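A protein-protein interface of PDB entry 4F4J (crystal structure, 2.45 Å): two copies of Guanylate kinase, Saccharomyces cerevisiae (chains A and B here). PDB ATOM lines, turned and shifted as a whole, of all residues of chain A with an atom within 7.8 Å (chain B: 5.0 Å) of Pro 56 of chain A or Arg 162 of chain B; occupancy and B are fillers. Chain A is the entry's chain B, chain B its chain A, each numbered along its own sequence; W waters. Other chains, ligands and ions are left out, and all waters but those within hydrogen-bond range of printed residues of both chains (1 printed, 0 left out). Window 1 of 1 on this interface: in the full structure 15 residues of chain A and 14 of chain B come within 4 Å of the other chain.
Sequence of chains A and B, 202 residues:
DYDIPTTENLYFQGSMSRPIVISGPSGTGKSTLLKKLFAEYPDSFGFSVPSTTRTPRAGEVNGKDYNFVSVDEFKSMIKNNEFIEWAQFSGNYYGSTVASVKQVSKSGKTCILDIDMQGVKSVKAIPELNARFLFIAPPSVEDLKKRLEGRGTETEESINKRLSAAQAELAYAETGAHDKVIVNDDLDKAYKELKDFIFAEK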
ATOM      1  N   THR A  52      14.011 -14.469 -10.888  1.00  0.00           N
ATOM      2  CA  THR A  52      12.921 -15.283 -11.283  1.00  0.00           C
ATOM      3  C   THR A  52      13.198 -16.147 -12.503  1.00  0.00           C
ATOM      4  O   THR A  52      14.014 -15.825 -13.371  1.00  0.00           O
ATOM      5  CB  THR A  52      11.609 -14.458 -11.538  1.00  0.00           C
ATOM      6  OG1 THR A  52      10.557 -15.412 -11.719  1.00  0.00           O
ATOM      7  CG2 THR A  52      11.691 -13.594 -12.827  1.00  0.00           C
ATOM      8  N   THR A  53      12.478 -17.260 -12.580  1.00  0.00           N
ATOM      9  CA  THR A  53      12.616 -18.143 -13.729  1.00  0.00           C
ATOM     10  C   THR A  53      11.491 -17.885 -14.710  1.00  0.00           C
ATOM     11  O   THR A  53      11.430 -18.518 -15.766  1.00  0.00           O
ATOM     12  CB  THR A  53      12.567 -19.616 -13.321  1.00  0.00           C
ATOM     13  OG1 THR A  53      11.309 -19.890 -12.687  1.00  0.00           O
ATOM     14  CG2 THR A  53      13.710 -19.939 -12.387  1.00  0.00           C
ATOM     15  N   ARG A  54      10.594 -16.965 -14.387  1.00  0.00           N
ATOM     16  CA  ARG A  54       9.479 -16.765 -15.315  1.00  0.00           C
ATOM     17  C   ARG A  54       9.907 -15.884 -16.527  1.00  0.00           C
ATOM     18  O   ARG A  54      10.925 -15.204 -16.488  1.00  0.00           O
ATOM     19  CB  ARG A  54       8.232 -16.202 -14.618  1.00  0.00           C
ATOM     20  CG  ARG A  54       8.303 -14.744 -14.203  1.00  0.00           C
ATOM     21  CD  ARG A  54       6.950 -14.127 -14.551  1.00  0.00           C
ATOM     22  NE  ARG A  54       6.770 -12.834 -13.898  1.00  0.00           N
ATOM     23  CZ  ARG A  54       7.242 -11.671 -14.356  1.00  0.00           C
ATOM     24  NH1 ARG A  54       7.970 -11.639 -15.479  1.00  0.00           N
ATOM     25  NH2 ARG A  54       6.965 -10.530 -13.681  1.00  0.00           N
ATOM     26  N   THR A  55       9.129 -15.926 -17.587  1.00  0.00           N
ATOM     27  CA  THR A  55       9.358 -15.116 -18.749  1.00  0.00           C
ATOM     28  C   THR A  55       9.219 -13.573 -18.540  1.00  0.00           C
ATOM     29  O   THR A  55       8.316 -13.123 -17.835  1.00  0.00           O
ATOM     30  CB  THR A  55       8.409 -15.616 -19.865  1.00  0.00           C
ATOM     31  OG1 THR A  55       8.797 -16.960 -20.234  1.00  0.00           O
ATOM     32  CG2 THR A  55       8.471 -14.705 -21.115  1.00  0.00           C
ATOM     33  N   PRO A  56      10.124 -12.762 -19.120  1.00  0.00           N
ATOM     34  CA  PRO A  56       9.951 -11.325 -18.975  1.00  0.00           C
ATOM     35  C   PRO A  56       8.637 -10.906 -19.567  1.00  0.00           C
ATOM     36  O   PRO A  56       8.144 -11.582 -20.465  1.00  0.00           O
ATOM     37  CB  PRO A  56      11.107 -10.747 -19.781  1.00  0.00           C
ATOM     38  CG  PRO A  56      12.226 -11.742 -19.546  1.00  0.00           C
ATOM     39  CD  PRO A  56      11.496 -13.112 -19.556  1.00  0.00           C
ATOM     40  N   ARG A  57       8.047  -9.857 -19.002  1.00  0.00           N
ATOM     41  CA  ARG A  57       6.800  -9.280 -19.443  1.00  0.00           C
ATOM     42  C   ARG A  57       7.078  -7.904 -20.111  1.00  0.00           C
ATOM     43  O   ARG A  57       8.221  -7.336 -20.089  1.00  0.00           O
ATOM     44  CB  ARG A  57       5.821  -9.137 -18.246  1.00  0.00           C
ATOM     45  CG  ARG A  57       4.829 -10.229 -18.112  1.00  0.00           C
ATOM     46  CD  ARG A  57       4.854 -11.304 -16.945  1.00  0.00           C
ATOM     47  NE  ARG A  57       4.343 -10.838 -15.672  1.00  0.00           N
ATOM     48  CZ  ARG A  57       3.789 -11.611 -14.691  1.00  0.00           C
ATOM     49  NH1 ARG A  57       3.575 -12.937 -14.783  1.00  0.00           N
ATOM     50  NH2 ARG A  57       3.457 -11.014 -13.547  1.00  0.00           N
ATOM     51  N   ALA A  58       6.060  -7.331 -20.715  1.00  0.00           N
ATOM     52  CA  ALA A  58       6.311  -6.092 -21.440  1.00  0.00           C
ATOM     53  C   ALA A  58       6.843  -5.019 -20.497  1.00  0.00           C
ATOM     54  O   ALA A  58       6.261  -4.785 -19.414  1.00  0.00           O
ATOM     55  CB  ALA A  58       5.052  -5.610 -22.132  1.00  0.00           C
ATOM     56  N   GLY A  59       7.948  -4.371 -20.910  1.00  0.00           N
ATOM     57  CA  GLY A  59       8.543  -3.213 -20.201  1.00  0.00           C
ATOM     58  C   GLY A  59       9.590  -3.674 -19.204  1.00  0.00           C
ATOM     59  O   GLY A  59      10.256  -2.840 -18.550  1.00  0.00           O
ATOM     60  N   GLU A  60       9.754  -4.986 -19.056  1.00  0.00           N
ATOM     61  CA  GLU A  60      10.637  -5.464 -17.996  1.00  0.00           C
ATOM     62  C   GLU A  60      12.060  -5.480 -18.443  1.00  0.00           C
ATOM     63  O   GLU A  60      12.328  -5.907 -19.583  1.00  0.00           O
ATOM     64  CB  GLU A  60      10.198  -6.838 -17.463  1.00  0.00           C
ATOM     65  CG  GLU A  60       9.014  -6.683 -16.409  1.00  0.00           C
ATOM     66  CD  GLU A  60       8.514  -8.025 -15.847  1.00  0.00           C
ATOM     67  OE1 GLU A  60       8.884  -9.101 -16.367  1.00  0.00           O
ATOM     68  OE2 GLU A  60       7.733  -7.980 -14.885  1.00  0.00           O
ATOM     69  N   VAL A  61      12.947  -5.012 -17.566  1.00  0.00           N
ATOM     70  CA  VAL A  61      14.389  -4.961 -17.835  1.00  0.00           C
ATOM     71  C   VAL A  61      15.151  -5.882 -16.908  1.00  0.00           C
ATOM     72  O   VAL A  61      15.007  -5.816 -15.652  1.00  0.00           O
ATOM     73  CB  VAL A  61      14.965  -3.504 -17.651  1.00  0.00           C
ATOM     74  CG1 VAL A  61      16.513  -3.443 -17.871  1.00  0.00           C
ATOM     75  CG2 VAL A  61      14.259  -2.459 -18.630  1.00  0.00           C
ATOM     76  N   ASN A  62      15.945  -6.763 -17.502  1.00  0.00           N
ATOM     77  CA  ASN A  62      16.802  -7.639 -16.759  1.00  0.00           C
ATOM     78  C   ASN A  62      17.727  -6.781 -15.929  1.00  0.00           C
ATOM     79  O   ASN A  62      18.187  -5.739 -16.396  1.00  0.00           O
ATOM     80  CB  ASN A  62      17.602  -8.507 -17.693  1.00  0.00           C
ATOM     81  CG  ASN A  62      18.416  -9.607 -16.926  1.00  0.00           C
ATOM     82  OD1 ASN A  62      19.644  -9.712 -17.071  1.00  0.00           O
ATOM     83  ND2 ASN A  62      17.731 -10.411 -16.140  1.00  0.00           N
ATOM     84  N   GLY A  63      17.962  -7.185 -14.682  1.00  0.00           N
ATOM     85  CA  GLY A  63      18.904  -6.484 -13.808  1.00  0.00           C
ATOM     86  C   GLY A  63      18.212  -5.343 -13.095  1.00  0.00           C
ATOM     87  O   GLY A  63      18.761  -4.797 -12.163  1.00  0.00           O
ATOM     88  N   ASP A  65      14.051  -4.923 -13.154  1.00  0.00           N
ATOM     89  CA  ASP A  65      12.834  -5.526 -12.635  1.00  0.00           C
ATOM     90  C   ASP A  65      13.090  -6.886 -12.030  1.00  0.00           C
ATOM     91  O   ASP A  65      12.616  -7.173 -10.953  1.00  0.00           O
ATOM     92  CB  ASP A  65      11.792  -5.603 -13.752  1.00  0.00           C
ATOM     93  CG  ASP A  65      11.451  -4.183 -14.304  1.00  0.00           C
ATOM     94  OD1 ASP A  65      10.810  -3.446 -13.561  1.00  0.00           O
ATOM     95  OD2 ASP A  65      11.881  -3.802 -15.409  1.00  0.00           O
ATOM     96  N   TYR A  66      13.839  -7.734 -12.728  1.00  0.00           N
ATOM     97  CA  TYR A  66      14.107  -9.057 -12.255  1.00  0.00           C
ATOM     98  C   TYR A  66      15.485  -9.413 -12.755  1.00  0.00           C
ATOM     99  O   TYR A  66      15.928  -8.911 -13.821  1.00  0.00           O
ATOM    100  CB  TYR A  66      13.072 -10.101 -12.799  1.00  0.00           C
ATOM    101  CG  TYR A  66      11.780 -10.084 -12.064  1.00  0.00           C
ATOM    102  CD1 TYR A  66      10.735  -9.279 -12.503  1.00  0.00           C
ATOM    103  CD2 TYR A  66      11.612 -10.806 -10.872  1.00  0.00           C
ATOM    104  CE1 TYR A  66       9.542  -9.195 -11.793  1.00  0.00           C
ATOM    105  CE2 TYR A  66      10.412 -10.746 -10.160  1.00  0.00           C
ATOM    106  CZ  TYR A  66       9.375  -9.935 -10.639  1.00  0.00           C
ATOM    107  OH  TYR A  66       8.171  -9.801  -9.956  1.00  0.00           O
ATOM    108  N   PHE A  68      16.566 -12.433 -14.419  1.00  0.00           N
ATOM    109  CA  PHE A  68      15.882 -13.549 -15.032  1.00  0.00           C
ATOM    110  C   PHE A  68      16.845 -14.646 -15.288  1.00  0.00           C
ATOM    111  O   PHE A  68      17.691 -14.511 -16.193  1.00  0.00           O
ATOM    112  CB  PHE A  68      15.308 -13.134 -16.368  1.00  0.00           C
ATOM    113  CG  PHE A  68      14.150 -12.173 -16.268  1.00  0.00           C
ATOM    114  CD1 PHE A  68      12.860 -12.632 -15.919  1.00  0.00           C
ATOM    115  CD2 PHE A  68      14.326 -10.829 -16.543  1.00  0.00           C
ATOM    116  CE1 PHE A  68      11.760 -11.768 -15.846  1.00  0.00           C
ATOM    117  CE2 PHE A  68      13.226  -9.931 -16.462  1.00  0.00           C
ATOM    118  CZ  PHE A  68      11.930 -10.414 -16.121  1.00  0.00           C
ATOM    119  N   VAL A  69      16.714 -15.741 -14.546  1.00  0.00           N
ATOM    120  CA  VAL A  69      17.641 -16.871 -14.643  1.00  0.00           C
ATOM    121  C   VAL A  69      16.874 -18.159 -14.976  1.00  0.00           C
ATOM    122  O   VAL A  69      15.659 -18.187 -14.872  1.00  0.00           O
ATOM    123  CB  VAL A  69      18.403 -17.109 -13.310  1.00  0.00           C
ATOM    124  CG1 VAL A  69      19.188 -15.833 -12.844  1.00  0.00           C
ATOM    125  CG2 VAL A  69      17.422 -17.569 -12.233  1.00  0.00           C
ATOM    126  N   SER B  26       7.237  -9.803 -25.375  1.00  0.00           N
ATOM    127  CA  SER B  26       8.229  -9.059 -24.637  1.00  0.00           C
ATOM    128  C   SER B  26       9.441  -8.592 -25.495  1.00  0.00           C
ATOM    129  O   SER B  26      10.109  -9.392 -26.183  1.00  0.00           O
ATOM    130  CB  SER B  26       8.721 -10.010 -23.564  1.00  0.00           C
ATOM    131  OG  SER B  26       9.280  -9.233 -22.553  1.00  0.00           O
ATOM    132  N   GLY B  27       9.752  -7.311 -25.452  1.00  0.00           N
ATOM    133  CA  GLY B  27      10.983  -6.825 -26.102  1.00  0.00           C
ATOM    134  C   GLY B  27      10.730  -6.175 -27.449  1.00  0.00           C
ATOM    135  O   GLY B  27      11.641  -5.566 -28.031  1.00  0.00           O
ATOM    136  N   LEU B 144      14.222  -9.442 -33.284  1.00  0.00           N
ATOM    137  CA  LEU B 144      13.964  -9.243 -31.872  1.00  0.00           C
ATOM    138  C   LEU B 144      15.233  -9.578 -31.080  1.00  0.00           C
ATOM    139  O   LEU B 144      15.612  -8.845 -30.163  1.00  0.00           O
ATOM    140  CB  LEU B 144      12.768 -10.102 -31.430  1.00  0.00           C
ATOM    141  CG  LEU B 144      12.350 -10.055 -29.967  1.00  0.00           C
ATOM    142  CD1 LEU B 144      12.003  -8.673 -29.577  1.00  0.00           C
ATOM    143  CD2 LEU B 144      11.156 -10.982 -29.642  1.00  0.00           C
ATOM    144  N   LEU B 148      17.290  -6.759 -28.690  1.00  0.00           N
ATOM    145  CA  LEU B 148      17.462  -7.003 -27.251  1.00  0.00           C
ATOM    146  C   LEU B 148      18.938  -7.035 -26.929  1.00  0.00           C
ATOM    147  O   LEU B 148      19.368  -6.531 -25.882  1.00  0.00           O
ATOM    148  CB  LEU B 148      16.840  -8.349 -26.839  1.00  0.00           C
ATOM    149  CG  LEU B 148      15.331  -8.467 -26.769  1.00  0.00           C
ATOM    150  CD1 LEU B 148      14.899  -9.952 -27.064  1.00  0.00           C
ATOM    151  CD2 LEU B 148      14.809  -7.944 -25.386  1.00  0.00           C
ATOM    152  N   ARG B 151      20.151  -3.502 -26.310  1.00  0.00           N
ATOM    153  CA  ARG B 151      19.951  -2.963 -24.966  1.00  0.00           C
ATOM    154  C   ARG B 151      21.118  -3.482 -24.131  1.00  0.00           C
ATOM    155  O   ARG B 151      21.636  -4.614 -24.332  1.00  0.00           O
ATOM    156  CB  ARG B 151      18.568  -3.401 -24.435  1.00  0.00           C
ATOM    157  CG  ARG B 151      17.453  -2.568 -25.079  1.00  0.00           C
ATOM    158  CD  ARG B 151      16.157  -3.295 -25.248  1.00  0.00           C
ATOM    159  NE  ARG B 151      15.682  -3.872 -23.985  1.00  0.00           N
ATOM    160  CZ  ARG B 151      14.412  -4.233 -23.735  1.00  0.00           C
ATOM    161  NH1 ARG B 151      13.466  -4.072 -24.658  1.00  0.00           N
ATOM    162  NH2 ARG B 151      14.099  -4.756 -22.554  1.00  0.00           N
ATOM    163  N   GLU B 154      20.433  -7.273 -21.077  1.00  0.00           N
ATOM    164  CA  GLU B 154      19.875  -8.588 -21.228  1.00  0.00           C
ATOM    165  C   GLU B 154      20.966  -9.613 -21.260  1.00  0.00           C
ATOM    166  O   GLU B 154      22.033  -9.361 -21.752  1.00  0.00           O
ATOM    167  CB  GLU B 154      19.046  -8.601 -22.491  1.00  0.00           C
ATOM    168  CG  GLU B 154      17.964  -7.505 -22.465  1.00  0.00           C
ATOM    169  CD  GLU B 154      16.989  -7.693 -21.256  1.00  0.00           C
ATOM    170  OE1 GLU B 154      16.716  -6.686 -20.492  1.00  0.00           O
ATOM    171  OE2 GLU B 154      16.559  -8.886 -21.086  1.00  0.00           O
ATOM    172  N   SER B 158      17.930 -14.270 -20.515  1.00  0.00           N
ATOM    173  CA  SER B 158      16.781 -13.439 -20.522  1.00  0.00           C
ATOM    174  C   SER B 158      16.293 -13.256 -21.948  1.00  0.00           C
ATOM    175  O   SER B 158      15.096 -13.277 -22.183  1.00  0.00           O
ATOM    176  CB  SER B 158      17.038 -12.140 -19.775  1.00  0.00           C
ATOM    177  OG  SER B 158      17.666 -11.174 -20.562  1.00  0.00           O
ATOM    178  N   ILE B 159      17.210 -13.144 -22.903  1.00  0.00           N
ATOM    179  CA  ILE B 159      16.855 -13.090 -24.335  1.00  0.00           C
ATOM    180  C   ILE B 159      16.214 -14.406 -24.777  1.00  0.00           C
ATOM    181  O   ILE B 159      15.147 -14.398 -25.380  1.00  0.00           O
ATOM    182  CB  ILE B 159      18.094 -12.826 -25.177  1.00  0.00           C
ATOM    183  CG1 ILE B 159      18.470 -11.365 -25.062  1.00  0.00           C
ATOM    184  CG2 ILE B 159      17.929 -13.246 -26.636  1.00  0.00           C
ATOM    185  CD1 ILE B 159      19.942 -11.139 -25.330  1.00  0.00           C
ATOM    186  N   ASN B 160      16.856 -15.525 -24.475  1.00  0.00           N
ATOM    187  CA  ASN B 160      16.300 -16.818 -24.862  1.00  0.00           C
ATOM    188  C   ASN B 160      14.833 -16.985 -24.411  1.00  0.00           C
ATOM    189  O   ASN B 160      14.001 -17.411 -25.200  1.00  0.00           O
ATOM    190  CB  ASN B 160      17.212 -18.016 -24.422  1.00  0.00           C
ATOM    191  CG  ASN B 160      18.536 -18.139 -25.338  1.00  0.00           C
ATOM    192  OD1 ASN B 160      18.684 -17.427 -26.377  1.00  0.00           O
ATOM    193  ND2 ASN B 160      19.496 -19.022 -24.915  1.00  0.00           N
ATOM    194  N   LYS B 161      14.526 -16.628 -23.168  1.00  0.00           N
ATOM    195  CA  LYS B 161      13.181 -16.812 -22.674  1.00  0.00           C
ATOM    196  C   LYS B 161      12.244 -16.000 -23.552  1.00  0.00           C
ATOM    197  O   LYS B 161      11.174 -16.456 -23.948  1.00  0.00           O
ATOM    198  CB  LYS B 161      13.043 -16.344 -21.225  1.00  0.00           C
ATOM    199  CG  LYS B 161      13.501 -17.346 -20.170  1.00  0.00           C
ATOM    200  CD  LYS B 161      13.344 -16.754 -18.757  1.00  0.00           C
ATOM    201  CE  LYS B 161      13.963 -17.686 -17.645  1.00  0.00           C
ATOM    202  NZ  LYS B 161      13.418 -19.045 -17.947  1.00  0.00           N
ATOM    203  N   ARG B 162      12.657 -14.808 -23.919  1.00  0.00           N
ATOM    204  CA  ARG B 162      11.737 -14.000 -24.699  1.00  0.00           C
ATOM    205  C   ARG B 162      11.550 -14.549 -26.113  1.00  0.00           C
ATOM    206  O   ARG B 162      10.423 -14.501 -26.653  1.00  0.00           O
ATOM    207  CB  ARG B 162      12.270 -12.610 -24.811  1.00  0.00           C
ATOM    208  CG  ARG B 162      12.556 -11.998 -23.544  1.00  0.00           C
ATOM    209  CD  ARG B 162      12.760 -10.509 -23.781  1.00  0.00           C
ATOM    210  NE  ARG B 162      13.468  -9.841 -22.664  1.00  0.00           N
ATOM    211  CZ  ARG B 162      12.958  -8.802 -22.008  1.00  0.00           C
ATOM    212  NH1 ARG B 162      11.744  -8.311 -22.329  1.00  0.00           N
ATOM    213  NH2 ARG B 162      13.650  -8.252 -21.057  1.00  0.00           N
ATOM    214  N   LEU B 163      12.645 -15.054 -26.695  1.00  0.00           N
ATOM    215  CA  LEU B 163      12.653 -15.538 -28.092  1.00  0.00           C
ATOM    216  C   LEU B 163      11.691 -16.718 -28.221  1.00  0.00           C
ATOM    217  O   LEU B 163      10.854 -16.759 -29.111  1.00  0.00           O
ATOM    218  CB  LEU B 163      14.056 -15.970 -28.536  1.00  0.00           C
ATOM    219  CG  LEU B 163      15.094 -14.824 -28.617  1.00  0.00           C
ATOM    220  CD1 LEU B 163      16.400 -15.315 -29.324  1.00  0.00           C
ATOM    221  CD2 LEU B 163      14.518 -13.653 -29.316  1.00  0.00           C
ATOM    222  N   SER B 164      11.780 -17.648 -27.303  1.00  0.00           N
ATOM    223  CA  SER B 164      10.935 -18.773 -27.454  1.00  0.00           C
ATOM    224  C   SER B 164       9.460 -18.379 -27.152  1.00  0.00           C
ATOM    225  O   SER B 164       8.563 -18.904 -27.757  1.00  0.00           O
ATOM    226  CB  SER B 164      11.466 -19.988 -26.663  1.00  0.00           C
ATOM    227  OG  SER B 164      11.610 -19.689 -25.291  1.00  0.00           O
ATOM    228  N   ALA B 165       9.221 -17.395 -26.302  1.00  0.00           N
ATOM    229  CA  ALA B 165       7.874 -16.945 -26.109  1.00  0.00           C
ATOM    230  C   ALA B 165       7.362 -16.190 -27.349  1.00  0.00           C
ATOM    231  O   ALA B 165       6.154 -16.242 -27.659  1.00  0.00           O
ATOM    232  CB  ALA B 165       7.735 -16.048 -24.815  1.00  0.00           C
ATOM    233  N   ALA B 166       8.252 -15.433 -27.989  1.00  0.00           N
ATOM    234  CA  ALA B 166       7.953 -14.798 -29.256  1.00  0.00           C
ATOM    235  C   ALA B 166       7.502 -15.846 -30.253  1.00  0.00           C
ATOM    236  O   ALA B 166       6.558 -15.604 -31.002  1.00  0.00           O
ATOM    237  CB  ALA B 166       9.173 -14.026 -29.820  1.00  0.00           C
ATOM    238  N   GLN B 167       8.188 -16.988 -30.277  1.00  0.00           N
ATOM    239  CA  GLN B 167       7.879 -18.016 -31.248  1.00  0.00           C
ATOM    240  C   GLN B 167       6.417 -18.463 -31.038  1.00  0.00           C
ATOM    241  O   GLN B 167       5.645 -18.515 -32.026  1.00  0.00           O
ATOM    242  CB  GLN B 167       8.814 -19.222 -31.060  1.00  0.00           C
ATOM    243  CG  GLN B 167       9.338 -19.781 -32.330  1.00  0.00           C
ATOM    244  CD  GLN B 167      10.791 -20.318 -32.138  1.00  0.00           C
ATOM    245  OE1 GLN B 167      11.768 -19.728 -32.671  1.00  0.00           O
ATOM    246  NE2 GLN B 167      10.934 -21.424 -31.350  1.00  0.00           N
HETATM  247  O   HOH W   1       9.819 -18.040 -22.514  1.00  0.00           O
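Printed residues of chain B within 4 Å of Thr 53 of chain A: Lys 161 (3.0 Å).
Of the printed residues of chain B, Pro 56 of chain A touches Ser 26, Lys 161 and Arg 162.
Of the printed residues of chain B, Glu 60 of chain A touches Arg 151 and Arg 162.
Printed residues of chain A within 4 Å of Ser 158 of chain B: Asn 62 and Phe 68.
Printed residues of chain A within 4 Å of Arg 162 of chain B: Pro 56 and Glu 60.
Among the printed residues, merely in contact across the chains: Arg 54 of chain A with Lys 161 of chain B (3.7 Å), Pro 56 of chain A with Lys 161 of chain B (3.95 Å), Pro 56 of chain A with Arg 162 of chain B (3.5 Å), Glu 60 of chain A with Arg 151 of chain B (3.6 Å), Val 61 of chain A with Glu 154 of chain B (3.9 Å), Asn 62 of chain A with Ser 158 of chain B (3.9 Å), Phe 68 of chain A with Ser 158 of chain B (3.9 Å) and Val 69 of chain A with Lys 161 of chain B (3.3 Å).
No position is printed for both chains.
Of the 13 pairs that touch across the chains among the printed residues, none has its exchanged pair printed and touching as well.
Water W1 bridges the backbone carbonyl oxygen (O) of Lys 161 of chain B (2.5 Å) and the side-chain hydroxyl (OG1) of Thr 55 of chain A (2.7 Å).
Of the 16 printed residues of chain A, 9 touch a printed residue of chain B.
Hydrophobic or aromatic side chains of chain A that line the printed part of chain B: Pro 56 and Phe 68.
Among the printed residues, 13 pairs touch across the chains.
Among the printed residues, no Asp or Glu carboxylate lies within 4 Å of a Lys or Arg side-chain nitrogen of the other chain.
The side-chain hydroxyl of Ser 26 of chain B sits at hydrogen-bond distance from the backbone carbonyl oxygen of Pro 56 of chain A (3.3 Å).
The side-chain hydroxyl of Ser 26 of chain B sits at hydrogen-bond distance from the backbone carbonyl oxygen of Arg 57 of chain A (3.3 Å).
OE1 of Glu 154 of chain B is in hydrogen-bond range of N of Asn 62 of chain A, at 3.1 Å.
The backbone carbonyl oxygen (O) of Thr 53 of chain A sits at hydrogen-bond distance from the side-chain amino group (NZ) of Lys 161 of chain B, at 3.0 Å.
NH2 of Arg 162 of chain B lies within hydrogen-bond range of O of Glu 60 of chain A, at 3.1 Å.
The guanidinium group of Arg 162 of chain B is in hydrogen-bond range of the side-chain hydroxyl of Ser 26 of chain B (2.6 Å).
The side-chain carboxylate of Glu 154 of chain B lies within hydrogen-bond range of the side-chain hydroxyl of Ser 158 of chain B, 2.6 Å away.
The backbone NH of Val 69 of chain A is in hydrogen-bond range of the backbone carbonyl oxygen of Thr 52 of chain A (2.9 Å).
The guanidinium group (NH1) of Arg 54 of chain A is in salt-bridge range of the side-chain carboxylate (OE1) of Glu 60 of chain A, at 2.8 Å.
N of Val 61 of chain A is in hydrogen-bond range of OD2 of Asp 65 of chain A, at 2.7 Å.
The backbone carbonyl oxygen (O) of Tyr 66 of chain A lies within hydrogen-bond range of the side-chain amide nitrogen (ND2) of Asn 62 of chain A, 3.3 Å away.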
